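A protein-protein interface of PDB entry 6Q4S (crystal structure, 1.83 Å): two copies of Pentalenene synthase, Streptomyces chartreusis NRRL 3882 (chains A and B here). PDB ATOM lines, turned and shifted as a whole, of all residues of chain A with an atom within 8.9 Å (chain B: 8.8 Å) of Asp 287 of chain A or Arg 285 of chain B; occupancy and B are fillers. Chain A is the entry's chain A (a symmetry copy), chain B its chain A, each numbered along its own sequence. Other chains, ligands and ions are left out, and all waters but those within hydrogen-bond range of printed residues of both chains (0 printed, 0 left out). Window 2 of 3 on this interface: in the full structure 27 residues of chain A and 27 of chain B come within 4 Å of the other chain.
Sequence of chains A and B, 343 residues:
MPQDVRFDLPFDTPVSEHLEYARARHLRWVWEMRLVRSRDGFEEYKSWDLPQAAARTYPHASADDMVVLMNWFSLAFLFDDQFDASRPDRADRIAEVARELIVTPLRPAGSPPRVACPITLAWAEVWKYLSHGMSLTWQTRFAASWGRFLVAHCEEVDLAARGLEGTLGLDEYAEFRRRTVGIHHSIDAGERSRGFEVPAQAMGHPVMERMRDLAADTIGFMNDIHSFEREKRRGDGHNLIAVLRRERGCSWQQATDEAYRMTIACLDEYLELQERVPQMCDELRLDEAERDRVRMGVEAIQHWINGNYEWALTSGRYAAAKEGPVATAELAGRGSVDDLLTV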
ATOM      1  N   PRO A 199     -26.358   2.169  -3.016  1.00  0.00           N
ATOM      2  CA  PRO A 199     -27.464   2.497  -2.082  1.00  0.00           C
ATOM      3  C   PRO A 199     -28.533   3.321  -2.723  1.00  0.00           C
ATOM      4  O   PRO A 199     -28.213   4.326  -3.407  1.00  0.00           O
ATOM      5  CB  PRO A 199     -26.766   3.249  -0.934  1.00  0.00           C
ATOM      6  CG  PRO A 199     -25.416   2.601  -0.917  1.00  0.00           C
ATOM      7  CD  PRO A 199     -25.047   2.369  -2.375  1.00  0.00           C
ATOM      8  N   GLN A 201     -30.797   5.456  -1.948  1.00  0.00           N
ATOM      9  CA  GLN A 201     -30.861   6.909  -1.685  1.00  0.00           C
ATOM     10  C   GLN A 201     -29.739   7.696  -2.401  1.00  0.00           C
ATOM     11  O   GLN A 201     -29.943   8.854  -2.693  1.00  0.00           O
ATOM     12  CB  GLN A 201     -30.902   7.224  -0.166  1.00  0.00           C
ATOM     13  CG  GLN A 201     -29.648   6.849   0.611  1.00  0.00           C
ATOM     14  CD  GLN A 201     -29.622   5.409   1.118  1.00  0.00           C
ATOM     15  OE1 GLN A 201     -29.792   4.445   0.369  1.00  0.00           O
ATOM     16  NE2 GLN A 201     -29.353   5.265   2.380  1.00  0.00           N
ATOM     17  N   CYS A 281     -22.342  11.755  -0.045  1.00  0.00           N
ATOM     18  CA  CYS A 281     -22.352  10.695   0.928  1.00  0.00           C
ATOM     19  C   CYS A 281     -22.508  11.223   2.337  1.00  0.00           C
ATOM     20  O   CYS A 281     -23.213  10.611   3.128  1.00  0.00           O
ATOM     21  CB  CYS A 281     -21.101   9.847   0.822  1.00  0.00           C
ATOM     22  SG  CYS A 281     -20.960   8.892  -0.707  1.00  0.00           S
ATOM     23  N   ASP A 282     -21.869  12.359   2.631  1.00  0.00           N
ATOM     24  CA  ASP A 282     -22.038  13.077   3.922  1.00  0.00           C
ATOM     25  C   ASP A 282     -23.481  13.563   4.123  1.00  0.00           C
ATOM     26  O   ASP A 282     -24.075  13.337   5.159  1.00  0.00           O
ATOM     27  CB  ASP A 282     -21.077  14.299   4.029  1.00  0.00           C
ATOM     28  CG  ASP A 282     -19.587  13.917   4.013  1.00  0.00           C
ATOM     29  OD1 ASP A 282     -19.222  12.744   4.214  1.00  0.00           O
ATOM     30  OD2 ASP A 282     -18.742  14.796   3.791  1.00  0.00           O
ATOM     31  N   LEU A 284     -26.206  12.466   2.776  1.00  0.00           N
ATOM     32  CA  LEU A 284     -26.993  11.233   2.967  1.00  0.00           C
ATOM     33  C   LEU A 284     -26.680  10.465   4.256  1.00  0.00           C
ATOM     34  O   LEU A 284     -27.435   9.577   4.595  1.00  0.00           O
ATOM     35  CB  LEU A 284     -26.777  10.274   1.765  1.00  0.00           C
ATOM     36  CG  LEU A 284     -27.363  10.805   0.447  1.00  0.00           C
ATOM     37  CD1 LEU A 284     -26.925   9.963  -0.728  1.00  0.00           C
ATOM     38  CD2 LEU A 284     -28.876  10.949   0.560  1.00  0.00           C
ATOM     39  N   ARG A 285     -25.576  10.785   4.943  1.00  0.00           N
ATOM     40  CA  ARG A 285     -25.135  10.092   6.187  1.00  0.00           C
ATOM     41  C   ARG A 285     -24.776   8.627   5.948  1.00  0.00           C
ATOM     42  O   ARG A 285     -25.092   7.743   6.744  1.00  0.00           O
ATOM     43  CB  ARG A 285     -26.168  10.180   7.316  1.00  0.00           C
ATOM     44  CG  ARG A 285     -26.736  11.553   7.560  1.00  0.00           C
ATOM     45  CD  ARG A 285     -27.726  11.477   8.711  1.00  0.00           C
ATOM     46  NE  ARG A 285     -29.056  12.001   8.364  1.00  0.00           N
ATOM     47  CZ  ARG A 285     -30.017  11.341   7.697  1.00  0.00           C
ATOM     48  NH1 ARG A 285     -29.840  10.104   7.233  1.00  0.00           N
ATOM     49  NH2 ARG A 285     -31.178  11.941   7.473  1.00  0.00           N
ATOM     50  N   LEU A 286     -24.110   8.350   4.851  1.00  0.00           N
ATOM     51  CA  LEU A 286     -23.790   6.967   4.565  1.00  0.00           C
ATOM     52  C   LEU A 286     -22.642   6.494   5.459  1.00  0.00           C
ATOM     53  O   LEU A 286     -21.719   7.242   5.712  1.00  0.00           O
ATOM     54  CB  LEU A 286     -23.442   6.760   3.077  1.00  0.00           C
ATOM     55  CG  LEU A 286     -24.429   7.281   2.036  1.00  0.00           C
ATOM     56  CD1 LEU A 286     -23.901   6.869   0.680  1.00  0.00           C
ATOM     57  CD2 LEU A 286     -25.845   6.769   2.274  1.00  0.00           C
ATOM     58  N   ASP A 287     -22.726   5.259   5.929  1.00  0.00           N
ATOM     59  CA  ASP A 287     -21.590   4.598   6.556  1.00  0.00           C
ATOM     60  C   ASP A 287     -20.532   4.228   5.528  1.00  0.00           C
ATOM     61  O   ASP A 287     -20.734   4.447   4.334  1.00  0.00           O
ATOM     62  CB  ASP A 287     -22.043   3.389   7.407  1.00  0.00           C
ATOM     63  CG  ASP A 287     -22.517   2.196   6.592  1.00  0.00           C
ATOM     64  OD1 ASP A 287     -21.945   1.810   5.533  1.00  0.00           O
ATOM     65  OD2 ASP A 287     -23.490   1.590   7.074  1.00  0.00           O
ATOM     66  N   GLU A 288     -19.441   3.615   5.986  1.00  0.00           N
ATOM     67  CA  GLU A 288     -18.264   3.392   5.145  1.00  0.00           C
ATOM     68  C   GLU A 288     -18.470   2.303   4.057  1.00  0.00           C
ATOM     69  O   GLU A 288     -17.944   2.429   2.950  1.00  0.00           O
ATOM     70  CB  GLU A 288     -17.006   3.172   6.032  1.00  0.00           C
ATOM     71  CG  GLU A 288     -16.180   1.900   5.818  1.00  0.00           C
ATOM     72  CD  GLU A 288     -15.290   1.569   7.028  1.00  0.00           C
ATOM     73  OE1 GLU A 288     -15.013   0.366   7.258  1.00  0.00           O
ATOM     74  OE2 GLU A 288     -14.881   2.501   7.777  1.00  0.00           O
ATOM     75  N   ALA A 289     -19.197   1.231   4.371  1.00  0.00           N
ATOM     76  CA  ALA A 289     -19.457   0.184   3.386  1.00  0.00           C
ATOM     77  C   ALA A 289     -20.460   0.686   2.281  1.00  0.00           C
ATOM     78  O   ALA A 289     -20.317   0.352   1.138  1.00  0.00           O
ATOM     79  CB  ALA A 289     -19.978  -1.063   4.074  1.00  0.00           C
ATOM     80  N   GLU A 290     -21.441   1.494   2.667  1.00  0.00           N
ATOM     81  CA  GLU A 290     -22.292   2.216   1.725  1.00  0.00           C
ATOM     82  C   GLU A 290     -21.442   3.150   0.817  1.00  0.00           C
ATOM     83  O   GLU A 290     -21.569   3.087  -0.425  1.00  0.00           O
ATOM     84  CB  GLU A 290     -23.383   2.998   2.465  1.00  0.00           C
ATOM     85  CG  GLU A 290     -24.413   2.051   3.087  1.00  0.00           C
ATOM     86  CD  GLU A 290     -25.374   2.682   4.094  1.00  0.00           C
ATOM     87  OE1 GLU A 290     -25.114   3.779   4.690  1.00  0.00           O
ATOM     88  OE2 GLU A 290     -26.427   2.055   4.291  1.00  0.00           O
ATOM     89  N   ARG A 291     -20.560   3.967   1.424  1.00  0.00           N
ATOM     90  CA  ARG A 291     -19.612   4.820   0.654  1.00  0.00           C
ATOM     91  C   ARG A 291     -18.846   4.045  -0.348  1.00  0.00           C
ATOM     92  O   ARG A 291     -18.650   4.516  -1.494  1.00  0.00           O
ATOM     93  CB  ARG A 291     -18.587   5.527   1.535  1.00  0.00           C
ATOM     94  CG  ARG A 291     -19.141   6.742   2.218  1.00  0.00           C
ATOM     95  CD  ARG A 291     -18.307   7.160   3.444  1.00  0.00           C
ATOM     96  NE  ARG A 291     -19.076   8.187   4.123  1.00  0.00           N
ATOM     97  CZ  ARG A 291     -19.020   9.496   3.877  1.00  0.00           C
ATOM     98  NH1 ARG A 291     -18.186  10.017   2.985  1.00  0.00           N
ATOM     99  NH2 ARG A 291     -19.840  10.295   4.531  1.00  0.00           N
ATOM    100  N   ASP A 292     -18.386   2.868   0.071  1.00  0.00           N
ATOM    101  CA  ASP A 292     -17.623   1.987  -0.809  1.00  0.00           C
ATOM    102  C   ASP A 292     -18.433   1.465  -2.024  1.00  0.00           C
ATOM    103  O   ASP A 292     -17.859   1.163  -3.102  1.00  0.00           O
ATOM    104  CB  ASP A 292     -17.092   0.784  -0.020  1.00  0.00           C
ATOM    105  CG  ASP A 292     -16.298  -0.179  -0.891  1.00  0.00           C
ATOM    106  OD1 ASP A 292     -15.279   0.280  -1.434  1.00  0.00           O
ATOM    107  OD2 ASP A 292     -16.688  -1.378  -1.073  1.00  0.00           O
ATOM    108  N   ARG A 293     -19.725   1.251  -1.805  1.00  0.00           N
ATOM    109  CA  ARG A 293     -20.631   0.762  -2.855  1.00  0.00           C
ATOM    110  C   ARG A 293     -20.910   1.910  -3.866  1.00  0.00           C
ATOM    111  O   ARG A 293     -20.928   1.665  -5.057  1.00  0.00           O
ATOM    112  CB  ARG A 293     -21.931   0.178  -2.237  1.00  0.00           C
ATOM    113  CG  ARG A 293     -21.710  -1.204  -1.560  1.00  0.00           C
ATOM    114  CD  ARG A 293     -22.756  -1.458  -0.452  1.00  0.00           C
ATOM    115  NE  ARG A 293     -24.118  -1.267  -0.968  1.00  0.00           N
ATOM    116  CZ  ARG A 293     -25.214  -1.000  -0.266  1.00  0.00           C
ATOM    117  NH1 ARG A 293     -25.203  -0.905   1.053  1.00  0.00           N
ATOM    118  NH2 ARG A 293     -26.371  -0.839  -0.906  1.00  0.00           N
ATOM    119  N   VAL A 294     -21.116   3.119  -3.348  1.00  0.00           N
ATOM    120  CA  VAL A 294     -21.136   4.355  -4.155  1.00  0.00           C
ATOM    121  C   VAL A 294     -19.921   4.512  -5.055  1.00  0.00           C
ATOM    122  O   VAL A 294     -20.034   4.616  -6.346  1.00  0.00           O
ATOM    123  CB  VAL A 294     -21.364   5.592  -3.277  1.00  0.00           C
ATOM    124  CG1 VAL A 294     -21.186   6.901  -4.076  1.00  0.00           C
ATOM    125  CG2 VAL A 294     -22.768   5.557  -2.721  1.00  0.00           C
ATOM    126  N   GLN B 201     -34.537   3.804   0.464  1.00  0.00           N
ATOM    127  CA  GLN B 201     -33.950   2.697   1.248  1.00  0.00           C
ATOM    128  C   GLN B 201     -34.996   1.961   2.117  1.00  0.00           C
ATOM    129  O   GLN B 201     -34.800   0.797   2.395  1.00  0.00           O
ATOM    130  CB  GLN B 201     -32.732   3.164   2.090  1.00  0.00           C
ATOM    131  CG  GLN B 201     -33.048   4.161   3.196  1.00  0.00           C
ATOM    132  CD  GLN B 201     -33.041   5.622   2.753  1.00  0.00           C
ATOM    133  OE1 GLN B 201     -33.718   6.024   1.804  1.00  0.00           O
ATOM    134  NE2 GLN B 201     -32.321   6.422   3.476  1.00  0.00           N
ATOM    135  N   HIS B 205     -36.376  -2.080   1.566  1.00  0.00           N
ATOM    136  CA  HIS B 205     -36.143  -2.891   2.761  1.00  0.00           C
ATOM    137  C   HIS B 205     -37.068  -4.146   2.773  1.00  0.00           C
ATOM    138  O   HIS B 205     -38.204  -4.075   2.307  1.00  0.00           O
ATOM    139  CB  HIS B 205     -36.359  -2.033   3.983  1.00  0.00           C
ATOM    140  CG  HIS B 205     -35.908  -2.661   5.255  1.00  0.00           C
ATOM    141  ND1 HIS B 205     -36.678  -3.583   5.935  1.00  0.00           N
ATOM    142  CD2 HIS B 205     -34.758  -2.526   5.961  1.00  0.00           C
ATOM    143  CE1 HIS B 205     -36.037  -3.968   7.023  1.00  0.00           C
ATOM    144  NE2 HIS B 205     -34.862  -3.358   7.053  1.00  0.00           N
ATOM    145  N   PRO B 278     -41.107   0.717  13.066  1.00  0.00           N
ATOM    146  CA  PRO B 278     -40.124   1.474  13.869  1.00  0.00           C
ATOM    147  C   PRO B 278     -38.746   0.811  13.954  1.00  0.00           C
ATOM    148  O   PRO B 278     -37.745   1.494  13.817  1.00  0.00           O
ATOM    149  CB  PRO B 278     -40.792   1.584  15.266  1.00  0.00           C
ATOM    150  CG  PRO B 278     -42.252   1.423  15.006  1.00  0.00           C
ATOM    151  CD  PRO B 278     -42.361   0.482  13.820  1.00  0.00           C
ATOM    152  N   GLN B 279     -38.655  -0.492  14.125  1.00  0.00           N
ATOM    153  CA  GLN B 279     -37.322  -1.126  14.126  1.00  0.00           C
ATOM    154  C   GLN B 279     -36.643  -0.986  12.746  1.00  0.00           C
ATOM    155  O   GLN B 279     -35.421  -0.885  12.664  1.00  0.00           O
ATOM    156  CB  GLN B 279     -37.402  -2.599  14.576  1.00  0.00           C
ATOM    157  CG  GLN B 279     -36.219  -3.506  14.229  1.00  0.00           C
ATOM    158  CD  GLN B 279     -36.504  -4.964  14.574  1.00  0.00           C
ATOM    159  OE1 GLN B 279     -36.511  -5.338  15.746  1.00  0.00           O
ATOM    160  NE2 GLN B 279     -36.744  -5.799  13.552  1.00  0.00           N
ATOM    161  N   MET B 280     -37.426  -1.055  11.663  1.00  0.00           N
ATOM    162  CA  MET B 280     -36.861  -0.918  10.322  1.00  0.00           C
ATOM    163  C   MET B 280     -36.233   0.484  10.193  1.00  0.00           C
ATOM    164  O   MET B 280     -35.116   0.619   9.708  1.00  0.00           O
ATOM    165  CB  MET B 280     -37.933  -1.144   9.223  1.00  0.00           C
ATOM    166  CG  MET B 280     -37.509  -0.690   7.812  1.00  0.00           C
ATOM    167  SD  MET B 280     -38.877  -0.813   6.648  1.00  0.00           S
ATOM    168  CE  MET B 280     -39.672   0.734   6.957  1.00  0.00           C
ATOM    169  N   CYS B 281     -36.968   1.500  10.641  1.00  0.00           N
ATOM    170  CA  CYS B 281     -36.505   2.861  10.577  1.00  0.00           C
ATOM    171  C   CYS B 281     -35.243   3.067  11.386  1.00  0.00           C
ATOM    172  O   CYS B 281     -34.364   3.795  10.943  1.00  0.00           O
ATOM    173  CB  CYS B 281     -37.581   3.825  11.032  1.00  0.00           C
ATOM    174  SG  CYS B 281     -39.026   3.916   9.949  1.00  0.00           S
ATOM    175  N   ASP B 282     -35.156   2.412  12.547  1.00  0.00           N
ATOM    176  CA  ASP B 282     -33.926   2.398  13.383  1.00  0.00           C
ATOM    177  C   ASP B 282     -32.746   1.737  12.655  1.00  0.00           C
ATOM    178  O   ASP B 282     -31.663   2.288  12.598  1.00  0.00           O
ATOM    179  CB  ASP B 282     -34.160   1.659  14.734  1.00  0.00           C
ATOM    180  CG  ASP B 282     -35.209   2.333  15.635  1.00  0.00           C
ATOM    181  OD1 ASP B 282     -35.578   3.504  15.426  1.00  0.00           O
ATOM    182  OD2 ASP B 282     -35.693   1.694  16.579  1.00  0.00           O
ATOM    183  N   GLU B 283     -32.945   0.545  12.124  1.00  0.00           N
ATOM    184  CA  GLU B 283     -31.886  -0.179  11.373  1.00  0.00           C
ATOM    185  C   GLU B 283     -31.369   0.605  10.136  1.00  0.00           C
ATOM    186  O   GLU B 283     -30.185   0.553   9.807  1.00  0.00           O
ATOM    187  CB  GLU B 283     -32.470  -1.536  10.994  1.00  0.00           C
ATOM    188  CG  GLU B 283     -31.775  -2.483  10.013  1.00  0.00           C
ATOM    189  CD  GLU B 283     -32.676  -3.717   9.736  1.00  0.00           C
ATOM    190  OE1 GLU B 283     -33.754  -3.867  10.391  1.00  0.00           O
ATOM    191  OE2 GLU B 283     -32.327  -4.546   8.862  1.00  0.00           O
ATOM    192  N   LEU B 284     -32.274   1.340   9.483  1.00  0.00           N
ATOM    193  CA  LEU B 284     -31.935   2.276   8.395  1.00  0.00           C
ATOM    194  C   LEU B 284     -31.373   3.623   8.860  1.00  0.00           C
ATOM    195  O   LEU B 284     -30.862   4.351   8.033  1.00  0.00           O
ATOM    196  CB  LEU B 284     -33.188   2.547   7.518  1.00  0.00           C
ATOM    197  CG  LEU B 284     -33.656   1.318   6.723  1.00  0.00           C
ATOM    198  CD1 LEU B 284     -35.000   1.558   6.080  1.00  0.00           C
ATOM    199  CD2 LEU B 284     -32.578   0.884   5.736  1.00  0.00           C
ATOM    200  N   ARG B 285     -31.491   3.959  10.151  1.00  0.00           N
ATOM    201  CA  ARG B 285     -31.025   5.253  10.725  1.00  0.00           C
ATOM    202  C   ARG B 285     -31.784   6.452  10.163  1.00  0.00           C
ATOM    203  O   ARG B 285     -31.214   7.506   9.875  1.00  0.00           O
ATOM    204  CB  ARG B 285     -29.520   5.478  10.543  1.00  0.00           C
ATOM    205  CG  ARG B 285     -28.647   4.307  10.909  1.00  0.00           C
ATOM    206  CD  ARG B 285     -27.193   4.691  10.690  1.00  0.00           C
ATOM    207  NE  ARG B 285     -26.478   3.759   9.805  1.00  0.00           N
ATOM    208  CZ  ARG B 285     -26.519   3.755   8.462  1.00  0.00           C
ATOM    209  NH1 ARG B 285     -27.272   4.609   7.771  1.00  0.00           N
ATOM    210  NH2 ARG B 285     -25.802   2.860   7.796  1.00  0.00           N
ATOM    211  N   LEU B 286     -33.079   6.313   9.998  1.00  0.00           N
ATOM    212  CA  LEU B 286     -33.828   7.411   9.424  1.00  0.00           C
ATOM    213  C   LEU B 286     -34.014   8.522  10.459  1.00  0.00           C
ATOM    214  O   LEU B 286     -34.231   8.242  11.621  1.00  0.00           O
ATOM    215  CB  LEU B 286     -35.191   6.944   8.875  1.00  0.00           C
ATOM    216  CG  LEU B 286     -35.204   5.760   7.913  1.00  0.00           C
ATOM    217  CD1 LEU B 286     -36.635   5.574   7.458  1.00  0.00           C
ATOM    218  CD2 LEU B 286     -34.256   5.962   6.736  1.00  0.00           C
ATOM    219  N   ASP B 287     -33.916   9.766  10.018  1.00  0.00           N
ATOM    220  CA  ASP B 287     -34.336  10.903  10.826  1.00  0.00           C
ATOM    221  C   ASP B 287     -35.851  10.969  10.938  1.00  0.00           C
ATOM    222  O   ASP B 287     -36.546  10.155  10.331  1.00  0.00           O
ATOM    223  CB  ASP B 287     -33.718  12.222  10.307  1.00  0.00           C
ATOM    224  CG  ASP B 287     -34.305  12.709   8.992  1.00  0.00           C
ATOM    225  OD1 ASP B 287     -35.539  12.656   8.724  1.00  0.00           O
ATOM    226  OD2 ASP B 287     -33.482  13.216   8.210  1.00  0.00           O
ATOM    227  N   GLU B 288     -36.355  11.972  11.657  1.00  0.00           N
ATOM    228  CA  GLU B 288     -37.773  12.035  12.015  1.00  0.00           C
ATOM    229  C   GLU B 288     -38.706  12.368  10.818  1.00  0.00           C
ATOM    230  O   GLU B 288     -39.822  11.851  10.742  1.00  0.00           O
ATOM    231  CB  GLU B 288     -37.972  12.956  13.250  1.00  0.00           C
ATOM    232  CG  GLU B 288     -38.962  14.120  13.136  1.00  0.00           C
ATOM    233  CD  GLU B 288     -38.718  15.204  14.200  1.00  0.00           C
ATOM    234  OE1 GLU B 288     -39.017  16.393  13.927  1.00  0.00           O
ATOM    235  OE2 GLU B 288     -38.200  14.886  15.309  1.00  0.00           O
ATOM    236  N   GLU B 290     -38.041  11.648   7.586  1.00  0.00           N
ATOM    237  CA  GLU B 290     -38.017  10.377   6.868  1.00  0.00           C
ATOM    238  C   GLU B 290     -38.996   9.357   7.517  1.00  0.00           C
ATOM    239  O   GLU B 290     -39.843   8.774   6.806  1.00  0.00           O
ATOM    240  CB  GLU B 290     -36.593   9.815   6.797  1.00  0.00           C
ATOM    241  CG  GLU B 290     -35.713  10.664   5.873  1.00  0.00           C
ATOM    242  CD  GLU B 290     -34.211  10.391   5.950  1.00  0.00           C
ATOM    243  OE1 GLU B 290     -33.672   9.825   6.958  1.00  0.00           O
ATOM    244  OE2 GLU B 290     -33.551  10.758   4.964  1.00  0.00           O
ATOM    245  N   ARG B 291     -38.911   9.182   8.849  1.00  0.00           N
ATOM    246  CA  ARG B 291     -39.869   8.322   9.597  1.00  0.00           C
ATOM    247  C   ARG B 291     -41.279   8.670   9.309  1.00  0.00           C
ATOM    248  O   ARG B 291     -42.130   7.764   9.142  1.00  0.00           O
ATOM    249  CB  ARG B 291     -39.701   8.406  11.111  1.00  0.00           C
ATOM    250  CG  ARG B 291     -38.553   7.585  11.619  1.00  0.00           C
ATOM    251  CD  ARG B 291     -38.079   8.035  13.015  1.00  0.00           C
ATOM    252  NE  ARG B 291     -36.844   7.318  13.272  1.00  0.00           N
ATOM    253  CZ  ARG B 291     -36.742   6.113  13.833  1.00  0.00           C
ATOM    254  NH1 ARG B 291     -37.799   5.445  14.278  1.00  0.00           N
ATOM    255  NH2 ARG B 291     -35.547   5.562  13.930  1.00  0.00           N
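Gln 201 of chain B touches its own counterpart, Gln 201 of chain A. Arg 285 of chain A touches its own counterpart, Arg 285 of chain B. Arg 285 of chain A touches Asp 287 of chain B, and with the chains exchanged Asp 287 of chain A touches Arg 285 of chain B. Arg 285 of chain A touches Glu 290 of chain B, and with the chains exchanged Glu 290 of chain A touches Arg 285 of chain B. Positions printed for both chains: 201, 281, 282, 284, 285, 286, 287, 288, 290 and 291. Of the 6 pairs that touch across the chains among the printed residues, 6 have their exchanged pair printed and touching as well.
Of chain B, only Arg 285 (2.7 Å) comes within 4 Å of Asp 287 of chain A. Of chain A, only Arg 285, Asp 287 and Glu 290 come within 4 Å of Arg 285 of chain B. Printed residues of chain A within 4 Å of Asp 287 of chain B: Arg 285. Of the printed residues of chain A, Glu 290 of chain B touches Arg 285 (3.3 Å). The nearest residue of chain B that does not touch Asp 287 of chain A is Glu 283 of chain B (7.3 Å). The nearest residue of chain A that does not touch Arg 285 of chain B is Leu 286 of chain A (5.3 Å). The nearest printed residue of chain B that does not touch Gln 201 of chain A is Arg 285 of chain B (5.8 Å).
Among the printed residues, merely in contact across the chains: Arg 285 of chain A with Arg 285 of chain B (3.95 Å).
NH2 of Arg 285 of chain B is in salt-bridge range of OD2 of Asp 287 of chain A (2.7 Å). The guanidinium group (NH2) of Arg 285 of chain A is in salt-bridge range of the side-chain carboxylate (OE1) of Glu 290 of chain B, 3.3 Å away. NE2 of Gln 201 of chain B lies close to NE2 of Gln 201 of chain A (3.4 Å). The guanidinium group (NH2) of Arg 285 of chain B is in salt-bridge range of the side-chain carboxylate (OE1) of Glu 290 of chain A (3.3 Å). The guanidinium group (NH2) of Arg 285 of chain A lies within salt-bridge range of the side-chain carboxylate (OD2) of Asp 287 of chain B.
Of the 15 printed residues of chain B, 4 touch a printed residue of chain A. Printed residues of chain B that touch a printed residue of chain A: Gln 201, Arg 285, Asp 287 and Glu 290. Along chain A the printed residues that touch a printed residue of chain B span positions 201 to 290. Among the printed residues, 6 pairs touch across the chains. Among the printed residues, Asp or Glu carboxylates within 4 Å of a Lys or Arg side-chain nitrogen of the other chain: Arg 285 of chain A with Asp 287 of chain B (2.7 Å), Arg 285 of chain A with Glu 290 of chain B (3.3 Å), Asp 287 of chain A with Arg 285 of chain B (2.7 Å) and Glu 290 of chain A with Arg 285 of chain B (3.3 Å).
The backbone NH (N) of Glu 290 of chain B lies within hydrogen-bond range of the side-chain carboxylate (OD1) of Asp 287 of chain B, at 2.9 Å. N of Glu 290 of chain A lies within hydrogen-bond range of OD1 of Asp 287 of chain A, 2.9 Å away. The backbone NH (N) of Ala 289 of chain A lies within hydrogen-bond range of the side-chain carboxylate (OD1) of Asp 287 of chain A (3.0 Å).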
